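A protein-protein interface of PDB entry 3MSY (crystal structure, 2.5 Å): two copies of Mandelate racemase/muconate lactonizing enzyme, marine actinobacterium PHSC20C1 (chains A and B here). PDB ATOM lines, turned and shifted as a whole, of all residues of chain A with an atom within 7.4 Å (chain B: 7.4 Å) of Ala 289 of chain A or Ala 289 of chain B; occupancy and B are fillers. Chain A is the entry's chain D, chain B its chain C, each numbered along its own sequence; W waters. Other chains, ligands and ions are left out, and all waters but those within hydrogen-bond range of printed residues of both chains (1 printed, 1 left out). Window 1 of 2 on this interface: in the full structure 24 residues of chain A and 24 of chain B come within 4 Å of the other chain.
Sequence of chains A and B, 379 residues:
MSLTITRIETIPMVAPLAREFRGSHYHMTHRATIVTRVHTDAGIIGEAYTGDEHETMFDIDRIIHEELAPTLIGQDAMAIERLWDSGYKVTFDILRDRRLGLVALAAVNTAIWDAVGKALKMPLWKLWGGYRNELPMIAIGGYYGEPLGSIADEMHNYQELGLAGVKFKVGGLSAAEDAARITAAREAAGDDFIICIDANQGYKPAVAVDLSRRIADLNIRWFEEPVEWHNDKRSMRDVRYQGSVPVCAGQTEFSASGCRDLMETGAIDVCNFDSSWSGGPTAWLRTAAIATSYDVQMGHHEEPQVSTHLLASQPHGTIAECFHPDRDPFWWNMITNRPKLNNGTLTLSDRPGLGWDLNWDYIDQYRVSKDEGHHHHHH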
ATOM      1  N   ALA A 256      22.842  18.912  10.186  1.00  0.00           N
ATOM      2  CA  ALA A 256      22.074  17.845   9.560  1.00  0.00           C
ATOM      3  C   ALA A 256      22.453  17.775   8.082  1.00  0.00           C
ATOM      4  O   ALA A 256      22.440  16.704   7.485  1.00  0.00           O
ATOM      5  CB  ALA A 256      20.582  18.114   9.717  1.00  0.00           C
ATOM      6  N   ARG A 260      23.391  14.673   6.022  1.00  0.00           N
ATOM      7  CA  ARG A 260      22.645  14.392   4.811  1.00  0.00           C
ATOM      8  C   ARG A 260      23.674  14.051   3.717  1.00  0.00           C
ATOM      9  O   ARG A 260      23.439  13.155   2.887  1.00  0.00           O
ATOM     10  CB  ARG A 260      21.789  15.614   4.432  1.00  0.00           C
ATOM     11  CG  ARG A 260      21.117  15.523   3.087  1.00  0.00           C
ATOM     12  CD  ARG A 260      20.282  16.777   2.716  1.00  0.00           C
ATOM     13  NE  ARG A 260      21.031  18.043   2.687  1.00  0.00           N
ATOM     14  CZ  ARG A 260      22.253  18.174   2.182  1.00  0.00           C
ATOM     15  NH1 ARG A 260      22.864  17.116   1.656  1.00  0.00           N
ATOM     16  NH2 ARG A 260      22.879  19.347   2.232  1.00  0.00           N
ATOM     17  N   MET A 263      24.997  10.597   3.932  1.00  0.00           N
ATOM     18  CA  MET A 263      23.963   9.681   3.461  1.00  0.00           C
ATOM     19  C   MET A 263      23.884   9.640   1.940  1.00  0.00           C
ATOM     20  O   MET A 263      23.851   8.559   1.340  1.00  0.00           O
ATOM     21  CB  MET A 263      22.608  10.065   4.077  1.00  0.00           C
ATOM     22  CG  MET A 263      22.573   9.766   5.567  1.00  0.00           C
ATOM     23  SD  MET A 263      20.953  10.315   6.508  1.00  0.00           S
ATOM     24  CE  MET A 263      21.762  11.026   8.150  1.00  0.00           C
ATOM     25  N   THR A 282      16.580  19.621  18.848  1.00  0.00           N
ATOM     26  CA  THR A 282      15.908  20.139  17.668  1.00  0.00           C
ATOM     27  C   THR A 282      16.692  19.790  16.393  1.00  0.00           C
ATOM     28  O   THR A 282      16.106  19.396  15.372  1.00  0.00           O
ATOM     29  CB  THR A 282      15.697  21.679  17.773  1.00  0.00           C
ATOM     30  OG1 THR A 282      14.830  21.969  18.881  1.00  0.00           O
ATOM     31  CG2 THR A 282      15.063  22.228  16.500  1.00  0.00           C
ATOM     32  N   ALA A 283      18.016  19.908  16.452  1.00  0.00           N
ATOM     33  CA  ALA A 283      18.834  19.582  15.292  1.00  0.00           C
ATOM     34  C   ALA A 283      18.907  18.073  15.045  1.00  0.00           C
ATOM     35  O   ALA A 283      18.714  17.611  13.917  1.00  0.00           O
ATOM     36  CB  ALA A 283      20.246  20.159  15.457  1.00  0.00           C
ATOM     37  N   TRP A 284      19.180  17.309  16.101  1.00  0.00           N
ATOM     38  CA  TRP A 284      19.302  15.859  15.980  1.00  0.00           C
ATOM     39  C   TRP A 284      18.034  15.195  15.428  1.00  0.00           C
ATOM     40  O   TRP A 284      18.119  14.223  14.684  1.00  0.00           O
ATOM     41  CB  TRP A 284      19.654  15.248  17.337  1.00  0.00           C
ATOM     42  CG  TRP A 284      20.042  13.793  17.279  1.00  0.00           C
ATOM     43  CD1 TRP A 284      21.306  13.285  17.216  1.00  0.00           C
ATOM     44  CD2 TRP A 284      19.161  12.665  17.347  1.00  0.00           C
ATOM     45  NE1 TRP A 284      21.272  11.911  17.249  1.00  0.00           N
ATOM     46  CE2 TRP A 284      19.968  11.503  17.329  1.00  0.00           C
ATOM     47  CE3 TRP A 284      17.768  12.521  17.424  1.00  0.00           C
ATOM     48  CZ2 TRP A 284      19.425  10.211  17.386  1.00  0.00           C
ATOM     49  CZ3 TRP A 284      17.230  11.240  17.479  1.00  0.00           C
ATOM     50  CH2 TRP A 284      18.057  10.099  17.461  1.00  0.00           C
ATOM     51  N   LEU A 285      16.866  15.713  15.800  1.00  0.00           N
ATOM     52  CA  LEU A 285      15.606  15.152  15.319  1.00  0.00           C
ATOM     53  C   LEU A 285      15.413  15.343  13.805  1.00  0.00           C
ATOM     54  O   LEU A 285      14.771  14.527  13.151  1.00  0.00           O
ATOM     55  CB  LEU A 285      14.432  15.745  16.107  1.00  0.00           C
ATOM     56  CG  LEU A 285      14.325  15.162  17.526  1.00  0.00           C
ATOM     57  CD1 LEU A 285      13.392  15.995  18.379  1.00  0.00           C
ATOM     58  CD2 LEU A 285      13.826  13.722  17.453  1.00  0.00           C
ATOM     59  N   ARG A 286      15.974  16.418  13.259  1.00  0.00           N
ATOM     60  CA  ARG A 286      15.897  16.683  11.834  1.00  0.00           C
ATOM     61  C   ARG A 286      16.783  15.678  11.113  1.00  0.00           C
ATOM     62  O   ARG A 286      16.417  15.148  10.072  1.00  0.00           O
ATOM     63  CB  ARG A 286      16.372  18.102  11.535  1.00  0.00           C
ATOM     64  CG  ARG A 286      15.411  19.189  11.982  1.00  0.00           C
ATOM     65  CD  ARG A 286      16.065  20.552  11.843  1.00  0.00           C
ATOM     66  NE  ARG A 286      15.179  21.636  12.256  1.00  0.00           N
ATOM     67  CZ  ARG A 286      15.504  22.929  12.227  1.00  0.00           C
ATOM     68  NH1 ARG A 286      16.706  23.313  11.806  1.00  0.00           N
ATOM     69  NH2 ARG A 286      14.619  23.840  12.615  1.00  0.00           N
ATOM     70  N   THR A 287      17.958  15.416  11.676  1.00  0.00           N
ATOM     71  CA  THR A 287      18.883  14.454  11.096  1.00  0.00           C
ATOM     72  C   THR A 287      18.242  13.067  11.116  1.00  0.00           C
ATOM     73  O   THR A 287      18.465  12.249  10.219  1.00  0.00           O
ATOM     74  CB  THR A 287      20.202  14.374  11.908  1.00  0.00           C
ATOM     75  OG1 THR A 287      20.917  15.608  11.802  1.00  0.00           O
ATOM     76  CG2 THR A 287      21.081  13.249  11.385  1.00  0.00           C
ATOM     77  N   ALA A 288      17.455  12.810  12.157  1.00  0.00           N
ATOM     78  CA  ALA A 288      16.795  11.522  12.330  1.00  0.00           C
ATOM     79  C   ALA A 288      15.739  11.316  11.255  1.00  0.00           C
ATOM     80  O   ALA A 288      15.567  10.205  10.756  1.00  0.00           O
ATOM     81  CB  ALA A 288      16.162  11.425  13.739  1.00  0.00           C
ATOM     82  N   ALA A 289      15.044  12.394  10.906  1.00  0.00           N
ATOM     83  CA  ALA A 289      14.027  12.345   9.865  1.00  0.00           C
ATOM     84  C   ALA A 289      14.690  12.163   8.498  1.00  0.00           C
ATOM     85  O   ALA A 289      14.184  11.410   7.669  1.00  0.00           O
ATOM     86  CB  ALA A 289      13.198  13.615   9.883  1.00  0.00           C
ATOM     87  N   ILE A 290      15.813  12.852   8.262  1.00  0.00           N
ATOM     88  CA  ILE A 290      16.541  12.722   6.992  1.00  0.00           C
ATOM     89  C   ILE A 290      16.924  11.246   6.869  1.00  0.00           C
ATOM     90  O   ILE A 290      16.831  10.649   5.802  1.00  0.00           O
ATOM     91  CB  ILE A 290      17.916  13.504   6.953  1.00  0.00           C
ATOM     92  CG1 ILE A 290      17.813  14.876   7.620  1.00  0.00           C
ATOM     93  CG2 ILE A 290      18.390  13.643   5.508  1.00  0.00           C
ATOM     94  CD1 ILE A 290      17.195  15.933   6.784  1.00  0.00           C
ATOM     95  N   ALA A 291      17.365  10.680   7.990  1.00  0.00           N
ATOM     96  CA  ALA A 291      17.807   9.289   8.042  1.00  0.00           C
ATOM     97  C   ALA A 291      16.740   8.250   7.700  1.00  0.00           C
ATOM     98  O   ALA A 291      17.065   7.194   7.162  1.00  0.00           O
ATOM     99  CB  ALA A 291      18.418   8.988   9.407  1.00  0.00           C
ATOM    100  N   THR A 292      15.475   8.521   8.006  1.00  0.00           N
ATOM    101  CA  THR A 292      14.457   7.540   7.657  1.00  0.00           C
ATOM    102  C   THR A 292      14.258   7.503   6.138  1.00  0.00           C
ATOM    103  O   THR A 292      13.915   6.457   5.602  1.00  0.00           O
ATOM    104  CB  THR A 292      13.071   7.811   8.308  1.00  0.00           C
ATOM    105  OG1 THR A 292      12.476   8.964   7.705  1.00  0.00           O
ATOM    106  CG2 THR A 292      13.204   8.007   9.803  1.00  0.00           C
ATOM    107  N   SER A 293      14.476   8.624   5.447  1.00  0.00           N
ATOM    108  CA  SER A 293      14.299   8.636   3.988  1.00  0.00           C
ATOM    109  C   SER A 293      15.470   7.941   3.305  1.00  0.00           C
ATOM    110  O   SER A 293      15.443   7.678   2.093  1.00  0.00           O
ATOM    111  CB  SER A 293      14.166  10.063   3.444  1.00  0.00           C
ATOM    112  OG  SER A 293      15.422  10.716   3.356  1.00  0.00           O
ATOM    113  N   TYR A 294      16.495   7.640   4.095  1.00  0.00           N
ATOM    114  CA  TYR A 294      17.682   6.965   3.585  1.00  0.00           C
ATOM    115  C   TYR A 294      17.847   5.551   4.125  1.00  0.00           C
ATOM    116  O   TYR A 294      18.864   4.914   3.873  1.00  0.00           O
ATOM    117  CB  TYR A 294      18.926   7.753   3.951  1.00  0.00           C
ATOM    118  CG  TYR A 294      19.289   8.836   2.989  1.00  0.00           C
ATOM    119  CD1 TYR A 294      19.843   8.531   1.754  1.00  0.00           C
ATOM    120  CD2 TYR A 294      19.127  10.172   3.329  1.00  0.00           C
ATOM    121  CE1 TYR A 294      20.234   9.527   0.880  1.00  0.00           C
ATOM    122  CE2 TYR A 294      19.515  11.181   2.465  1.00  0.00           C
ATOM    123  CZ  TYR A 294      20.068  10.848   1.239  1.00  0.00           C
ATOM    124  OH  TYR A 294      20.445  11.833   0.368  1.00  0.00           O
ATOM    125  N   MET A 298      19.755   5.411  13.308  1.00  0.00           N
ATOM    126  CA  MET A 298      20.272   6.512  14.120  1.00  0.00           C
ATOM    127  C   MET A 298      21.009   6.020  15.351  1.00  0.00           C
ATOM    128  O   MET A 298      20.607   5.051  15.987  1.00  0.00           O
ATOM    129  CB  MET A 298      19.150   7.460  14.572  1.00  0.00           C
ATOM    130  CG  MET A 298      18.606   8.386  13.495  1.00  0.00           C
ATOM    131  SD  MET A 298      19.966   9.547  12.643  1.00  0.00           S
ATOM    132  CE  MET A 298      20.666  10.493  14.202  1.00  0.00           C
ATOM    133  N   GLN A 314      12.749   7.209  18.351  1.00  0.00           N
ATOM    134  CA  GLN A 314      12.837   6.893  16.931  1.00  0.00           C
ATOM    135  C   GLN A 314      12.745   5.413  16.600  1.00  0.00           C
ATOM    136  O   GLN A 314      13.423   4.585  17.218  1.00  0.00           O
ATOM    137  CB  GLN A 314      14.155   7.434  16.357  1.00  0.00           C
ATOM    138  CG  GLN A 314      14.346   8.924  16.529  1.00  0.00           C
ATOM    139  CD  GLN A 314      13.234   9.725  15.879  1.00  0.00           C
ATOM    140  OE1 GLN A 314      13.121   9.770  14.649  1.00  0.00           O
ATOM    141  NE2 GLN A 314      12.398  10.356  16.702  1.00  0.00           N
ATOM    142  N   HIS A 316      13.950   3.972  14.204  1.00  0.00           N
ATOM    143  CA  HIS A 316      15.224   3.543  13.658  1.00  0.00           C
ATOM    144  C   HIS A 316      16.384   3.840  14.614  1.00  0.00           C
ATOM    145  O   HIS A 316      17.529   3.987  14.190  1.00  0.00           O
ATOM    146  CB  HIS A 316      15.451   4.211  12.297  1.00  0.00           C
ATOM    147  CG  HIS A 316      15.414   5.710  12.339  1.00  0.00           C
ATOM    148  ND1 HIS A 316      14.555   6.414  13.155  1.00  0.00           N
ATOM    149  CD2 HIS A 316      16.107   6.637  11.635  1.00  0.00           C
ATOM    150  CE1 HIS A 316      14.721   7.709  12.954  1.00  0.00           C
ATOM    151  NE2 HIS A 316      15.655   7.870  12.037  1.00  0.00           N
ATOM    152  N   ALA B 256       8.674  10.865   1.588  1.00  0.00           N
ATOM    153  CA  ALA B 256       9.738  11.802   1.925  1.00  0.00           C
ATOM    154  C   ALA B 256      10.959  11.545   1.036  1.00  0.00           C
ATOM    155  O   ALA B 256      11.633  12.480   0.612  1.00  0.00           O
ATOM    156  CB  ALA B 256      10.126  11.654   3.427  1.00  0.00           C
ATOM    157  N   MET B 263      15.001  17.429  -4.172  1.00  0.00           N
ATOM    158  CA  MET B 263      15.929  18.403  -3.612  1.00  0.00           C
ATOM    159  C   MET B 263      17.382  18.091  -3.911  1.00  0.00           C
ATOM    160  O   MET B 263      18.199  19.000  -4.043  1.00  0.00           O
ATOM    161  CB  MET B 263      15.733  18.492  -2.100  1.00  0.00           C
ATOM    162  CG  MET B 263      14.384  19.032  -1.682  1.00  0.00           C
ATOM    163  SD  MET B 263      14.117  18.757   0.238  1.00  0.00           S
ATOM    164  CE  MET B 263      12.249  18.115   0.240  1.00  0.00           C
ATOM    165  N   THR B 282       2.865  13.157  10.117  1.00  0.00           N
ATOM    166  CA  THR B 282       4.088  12.501  10.552  1.00  0.00           C
ATOM    167  C   THR B 282       5.116  12.410   9.430  1.00  0.00           C
ATOM    168  O   THR B 282       6.310  12.609   9.647  1.00  0.00           O
ATOM    169  CB  THR B 282       3.781  11.098  11.100  1.00  0.00           C
ATOM    170  OG1 THR B 282       3.242  11.228  12.419  1.00  0.00           O
ATOM    171  CG2 THR B 282       5.039  10.233  11.140  1.00  0.00           C
ATOM    172  N   ALA B 283       4.646  12.114   8.226  1.00  0.00           N
ATOM    173  CA  ALA B 283       5.533  12.002   7.084  1.00  0.00           C
ATOM    174  C   ALA B 283       5.857  13.392   6.543  1.00  0.00           C
ATOM    175  O   ALA B 283       6.968  13.651   6.087  1.00  0.00           O
ATOM    176  CB  ALA B 283       4.877  11.151   6.000  1.00  0.00           C
ATOM    177  N   TRP B 284       4.883  14.289   6.598  1.00  0.00           N
ATOM    178  CA  TRP B 284       5.096  15.632   6.096  1.00  0.00           C
ATOM    179  C   TRP B 284       6.214  16.318   6.874  1.00  0.00           C
ATOM    180  O   TRP B 284       7.071  16.995   6.296  1.00  0.00           O
ATOM    181  CB  TRP B 284       3.821  16.462   6.224  1.00  0.00           C
ATOM    182  CG  TRP B 284       3.901  17.754   5.482  1.00  0.00           C
ATOM    183  CD1 TRP B 284       3.499  17.986   4.198  1.00  0.00           C
ATOM    184  CD2 TRP B 284       4.410  19.001   5.974  1.00  0.00           C
ATOM    185  NE1 TRP B 284       3.718  19.303   3.862  1.00  0.00           N
ATOM    186  CE2 TRP B 284       4.278  19.948   4.932  1.00  0.00           C
ATOM    187  CE3 TRP B 284       4.964  19.413   7.197  1.00  0.00           C
ATOM    188  CZ2 TRP B 284       4.678  21.284   5.076  1.00  0.00           C
ATOM    189  CZ3 TRP B 284       5.358  20.739   7.338  1.00  0.00           C
ATOM    190  CH2 TRP B 284       5.212  21.658   6.281  1.00  0.00           C
ATOM    191  N   LEU B 285       6.200  16.137   8.191  1.00  0.00           N
ATOM    192  CA  LEU B 285       7.189  16.770   9.045  1.00  0.00           C
ATOM    193  C   LEU B 285       8.569  16.200   8.813  1.00  0.00           C
ATOM    194  O   LEU B 285       9.561  16.875   9.045  1.00  0.00           O
ATOM    195  CB  LEU B 285       6.765  16.658  10.511  1.00  0.00           C
ATOM    196  CG  LEU B 285       5.507  17.503  10.778  1.00  0.00           C
ATOM    197  CD1 LEU B 285       4.857  17.086  12.083  1.00  0.00           C
ATOM    198  CD2 LEU B 285       5.857  18.998  10.787  1.00  0.00           C
ATOM    199  N   ARG B 286       8.634  14.963   8.335  1.00  0.00           N
ATOM    200  CA  ARG B 286       9.917  14.353   8.027  1.00  0.00           C
ATOM    201  C   ARG B 286      10.467  15.063   6.800  1.00  0.00           C
ATOM    202  O   ARG B 286      11.640  15.431   6.754  1.00  0.00           O
ATOM    203  CB  ARG B 286       9.752  12.858   7.743  1.00  0.00           C
ATOM    204  CG  ARG B 286       9.444  12.054   8.991  1.00  0.00           C
ATOM    205  CD  ARG B 286       9.344  10.571   8.722  1.00  0.00           C
ATOM    206  NE  ARG B 286       9.029   9.837   9.945  1.00  0.00           N
ATOM    207  CZ  ARG B 286       8.890   8.516  10.015  1.00  0.00           C
ATOM    208  NH1 ARG B 286       9.039   7.771   8.922  1.00  0.00           N
ATOM    209  NH2 ARG B 286       8.606   7.942  11.181  1.00  0.00           N
ATOM    210  N   THR B 287       9.596  15.252   5.813  1.00  0.00           N
ATOM    211  CA  THR B 287       9.934  15.936   4.577  1.00  0.00           C
ATOM    212  C   THR B 287      10.391  17.363   4.887  1.00  0.00           C
ATOM    213  O   THR B 287      11.416  17.821   4.369  1.00  0.00           O
ATOM    214  CB  THR B 287       8.715  15.987   3.634  1.00  0.00           C
ATOM    215  OG1 THR B 287       8.391  14.658   3.205  1.00  0.00           O
ATOM    216  CG2 THR B 287       9.002  16.840   2.425  1.00  0.00           C
ATOM    217  N   ALA B 288       9.621  18.062   5.722  1.00  0.00           N
ATOM    218  CA  ALA B 288       9.950  19.430   6.121  1.00  0.00           C
ATOM    219  C   ALA B 288      11.305  19.484   6.847  1.00  0.00           C
ATOM    220  O   ALA B 288      12.025  20.477   6.758  1.00  0.00           O
ATOM    221  CB  ALA B 288       8.861  19.987   7.012  1.00  0.00           C
ATOM    222  N   ALA B 289      11.645  18.424   7.573  1.00  0.00           N
ATOM    223  CA  ALA B 289      12.929  18.379   8.256  1.00  0.00           C
ATOM    224  C   ALA B 289      14.008  18.276   7.176  1.00  0.00           C
ATOM    225  O   ALA B 289      15.029  18.956   7.229  1.00  0.00           O
ATOM    226  CB  ALA B 289      12.998  17.178   9.169  1.00  0.00           C
ATOM    227  N   ILE B 290      13.778  17.415   6.193  1.00  0.00           N
ATOM    228  CA  ILE B 290      14.727  17.243   5.109  1.00  0.00           C
ATOM    229  C   ILE B 290      14.891  18.584   4.398  1.00  0.00           C
ATOM    230  O   ILE B 290      16.007  19.042   4.142  1.00  0.00           O
ATOM    231  CB  ILE B 290      14.229  16.167   4.105  1.00  0.00           C
ATOM    232  CG1 ILE B 290      14.214  14.798   4.784  1.00  0.00           C
ATOM    233  CG2 ILE B 290      15.115  16.146   2.867  1.00  0.00           C
ATOM    234  CD1 ILE B 290      13.561  13.693   3.959  1.00  0.00           C
ATOM    235  N   ALA B 291      13.767  19.214   4.089  1.00  0.00           N
ATOM    236  CA  ALA B 291      13.784  20.497   3.410  1.00  0.00           C
ATOM    237  C   ALA B 291      14.758  21.504   4.049  1.00  0.00           C
ATOM    238  O   ALA B 291      15.450  22.223   3.328  1.00  0.00           O
ATOM    239  CB  ALA B 291      12.376  21.074   3.371  1.00  0.00           C
ATOM    240  N   THR B 292      14.831  21.544   5.385  1.00  0.00           N
ATOM    241  CA  THR B 292      15.723  22.494   6.049  1.00  0.00           C
ATOM    242  C   THR B 292      17.203  22.277   5.723  1.00  0.00           C
ATOM    243  O   THR B 292      17.951  23.241   5.619  1.00  0.00           O
ATOM    244  CB  THR B 292      15.541  22.520   7.620  1.00  0.00           C
ATOM    245  OG1 THR B 292      16.057  21.323   8.217  1.00  0.00           O
ATOM    246  CG2 THR B 292      14.080  22.660   7.994  1.00  0.00           C
ATOM    247  N   SER B 293      17.627  21.027   5.545  1.00  0.00           N
ATOM    248  CA  SER B 293      19.030  20.751   5.240  1.00  0.00           C
ATOM    249  C   SER B 293      19.408  21.146   3.807  1.00  0.00           C
ATOM    250  O   SER B 293      20.582  21.324   3.487  1.00  0.00           O
ATOM    251  CB  SER B 293      19.349  19.268   5.481  1.00  0.00           C
ATOM    252  OG  SER B 293      18.775  18.441   4.494  1.00  0.00           O
ATOM    253  N   TYR B 294      18.408  21.281   2.943  1.00  0.00           N
ATOM    254  CA  TYR B 294      18.658  21.665   1.560  1.00  0.00           C
ATOM    255  C   TYR B 294      18.224  23.111   1.325  1.00  0.00           C
ATOM    256  O   TYR B 294      18.211  23.572   0.192  1.00  0.00           O
ATOM    257  CB  TYR B 294      17.869  20.771   0.607  1.00  0.00           C
ATOM    258  CG  TYR B 294      18.400  19.374   0.341  1.00  0.00           C
ATOM    259  CD1 TYR B 294      19.446  19.160  -0.558  1.00  0.00           C
ATOM    260  CD2 TYR B 294      17.754  18.253   0.871  1.00  0.00           C
ATOM    261  CE1 TYR B 294      19.826  17.866  -0.938  1.00  0.00           C
ATOM    262  CE2 TYR B 294      18.123  16.955   0.498  1.00  0.00           C
ATOM    263  CZ  TYR B 294      19.154  16.769  -0.409  1.00  0.00           C
ATOM    264  OH  TYR B 294      19.497  15.487  -0.797  1.00  0.00           O
ATOM    265  N   MET B 298       9.141  25.146   2.482  1.00  0.00           N
ATOM    266  CA  MET B 298       8.019  24.219   2.501  1.00  0.00           C
ATOM    267  C   MET B 298       6.722  24.928   2.138  1.00  0.00           C
ATOM    268  O   MET B 298       6.532  26.110   2.424  1.00  0.00           O
ATOM    269  CB  MET B 298       7.849  23.562   3.877  1.00  0.00           C
ATOM    270  CG  MET B 298       8.854  22.471   4.229  1.00  0.00           C
ATOM    271  SD  MET B 298       8.895  20.965   2.969  1.00  0.00           S
ATOM    272  CE  MET B 298       7.011  20.420   2.951  1.00  0.00           C
ATOM    273  N   GLN B 314       6.557  25.545  10.917  1.00  0.00           N
ATOM    274  CA  GLN B 314       7.920  25.473  10.410  1.00  0.00           C
ATOM    275  C   GLN B 314       8.551  26.833  10.105  1.00  0.00           C
ATOM    276  O   GLN B 314       7.895  27.752   9.611  1.00  0.00           O
ATOM    277  CB  GLN B 314       7.964  24.570   9.175  1.00  0.00           C
ATOM    278  CG  GLN B 314       7.453  23.154   9.444  1.00  0.00           C
ATOM    279  CD  GLN B 314       8.171  22.470  10.605  1.00  0.00           C
ATOM    280  OE1 GLN B 314       9.366  22.182  10.529  1.00  0.00           O
ATOM    281  NE2 GLN B 314       7.442  22.219  11.687  1.00  0.00           N
ATOM    282  N   HIS B 316      10.558  27.498   7.849  1.00  0.00           N
ATOM    283  CA  HIS B 316      10.673  27.660   6.405  1.00  0.00           C
ATOM    284  C   HIS B 316       9.330  27.481   5.693  1.00  0.00           C
ATOM    285  O   HIS B 316       9.281  27.273   4.476  1.00  0.00           O
ATOM    286  CB  HIS B 316      11.724  26.680   5.842  1.00  0.00           C
ATOM    287  CG  HIS B 316      11.503  25.250   6.237  1.00  0.00           C
ATOM    288  ND1 HIS B 316      11.042  24.881   7.486  1.00  0.00           N
ATOM    289  CD2 HIS B 316      11.719  24.096   5.562  1.00  0.00           C
ATOM    290  CE1 HIS B 316      10.982  23.564   7.560  1.00  0.00           C
ATOM    291  NE2 HIS B 316      11.389  23.064   6.407  1.00  0.00           N
HETATM  292  O   HOH W   1      18.172  21.484   9.412  1.00  0.00           O
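Among the printed residues, pairs that only touch across the chains: Arg 260 of chain A with Tyr 294 of chain B (3.1 Å), Arg 286 of chain A with Ala 289 of chain B (3.97 Å), Arg 286 of chain A with Thr 292 of chain B (3.7 Å), Ala 289 of chain A with Arg 286 of chain B (3.8 Å), Ala 289 of chain A with Ala 289 of chain B (3.6 Å), Ile 290 of chain A with Ala 289 of chain B (3.7 Å), Ile 290 of chain A with Ile 290 of chain B (3.3 Å), Ile 290 of chain A with Ser 293 of chain B (3.7 Å), Thr 292 of chain A with Arg 286 of chain B (3.7 Å), Ser 293 of chain A with Ile 290 of chain B (3.6 Å) and Tyr 294 of chain A with Tyr 294 of chain B (3.95 Å).
Thr 282 of chain A touches none of the printed residues of chain B. Ala 288 of chain A touches none of the printed residues of chain B. Ala 256 of chain B touches none of the printed residues of chain A. No residue of chain A comes within 4 Å of Ala 288 of chain B. Of chain A, only Arg 286 (3.97 Å), Ala 289 (3.6 Å) and Ile 290 (3.7 Å) come within 4 Å of Ala 289 of chain B. Of the printed residues of chain A, Ile 290 of chain B touches Ile 290 and Ser 293. Printed residues of chain A within 4 Å of Ser 293 of chain B: Arg 260 (2.9 Å) and Ile 290 (3.7 Å). The nearest printed residue of chain B that does not touch Arg 260 of chain A is Ile 290 of chain B (5.0 Å).
Water W1 bridges the side-chain hydroxyl of Thr 292 of chain B and the guanidinium group of Arg 286 of chain A.
O of Ala 289 of chain B lies within hydrogen-bond range of OG1 of Thr 292 of chain B, 2.8 Å away. O of Ala 289 of chain A lies within hydrogen-bond range of OG1 of Thr 292 of chain A, at 3.0 Å. The backbone carbonyl oxygen (O) of Ile 290 of chain A lies within hydrogen-bond range of the side-chain hydroxyl (OG) of Ser 293 of chain A (2.8 Å). The backbone carbonyl oxygen (O) of Ile 290 of chain B lies within hydrogen-bond range of the side-chain hydroxyl (OG) of Ser 293 of chain B, 2.9 Å away.
Printed residues of chain A that touch a printed residue of chain B: Arg 260, Arg 286, Ala 289, Ile 290, Thr 292, Ser 293 and Tyr 294. Hydrophobic or aromatic side chains of chain A within 4 Å of the printed part of chain B: Ala 289, Ile 290 and Tyr 294. Hydrophobic or aromatic side chains of chain B within 4 Å of the printed part of chain A: Ala 289, Ile 290 and Tyr 294. Along chain B the printed residues that touch a printed residue of chain A span positions 286 to 294. Among the printed residues, no Asp or Glu carboxylate lies within 4 Å of a Lys or Arg side-chain nitrogen of the other chain.
OG of Ser 293 of chain B sits close to NE of Arg 260 of chain A (2.9 Å).
Arg 286 of chain A touches Ala 289 of chain B, and with the chains exchanged Ala 289 of chain A touches Arg 286 of chain B. Arg 286 of chain A touches Thr 292 of chain B, and with the chains exchanged Thr 292 of chain A touches Arg 286 of chain B. Ala 289 of chain B touches its own counterpart, Ala 289 of chain A. Tyr 294 of chain B touches its own counterpart, Tyr 294 of chain A. Positions printed for both chains: 256, 263, 282, 283, 284, 285, 286, 287, 288, 289, 290, 291, 292, 293, 294, 298, 314 and 316.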
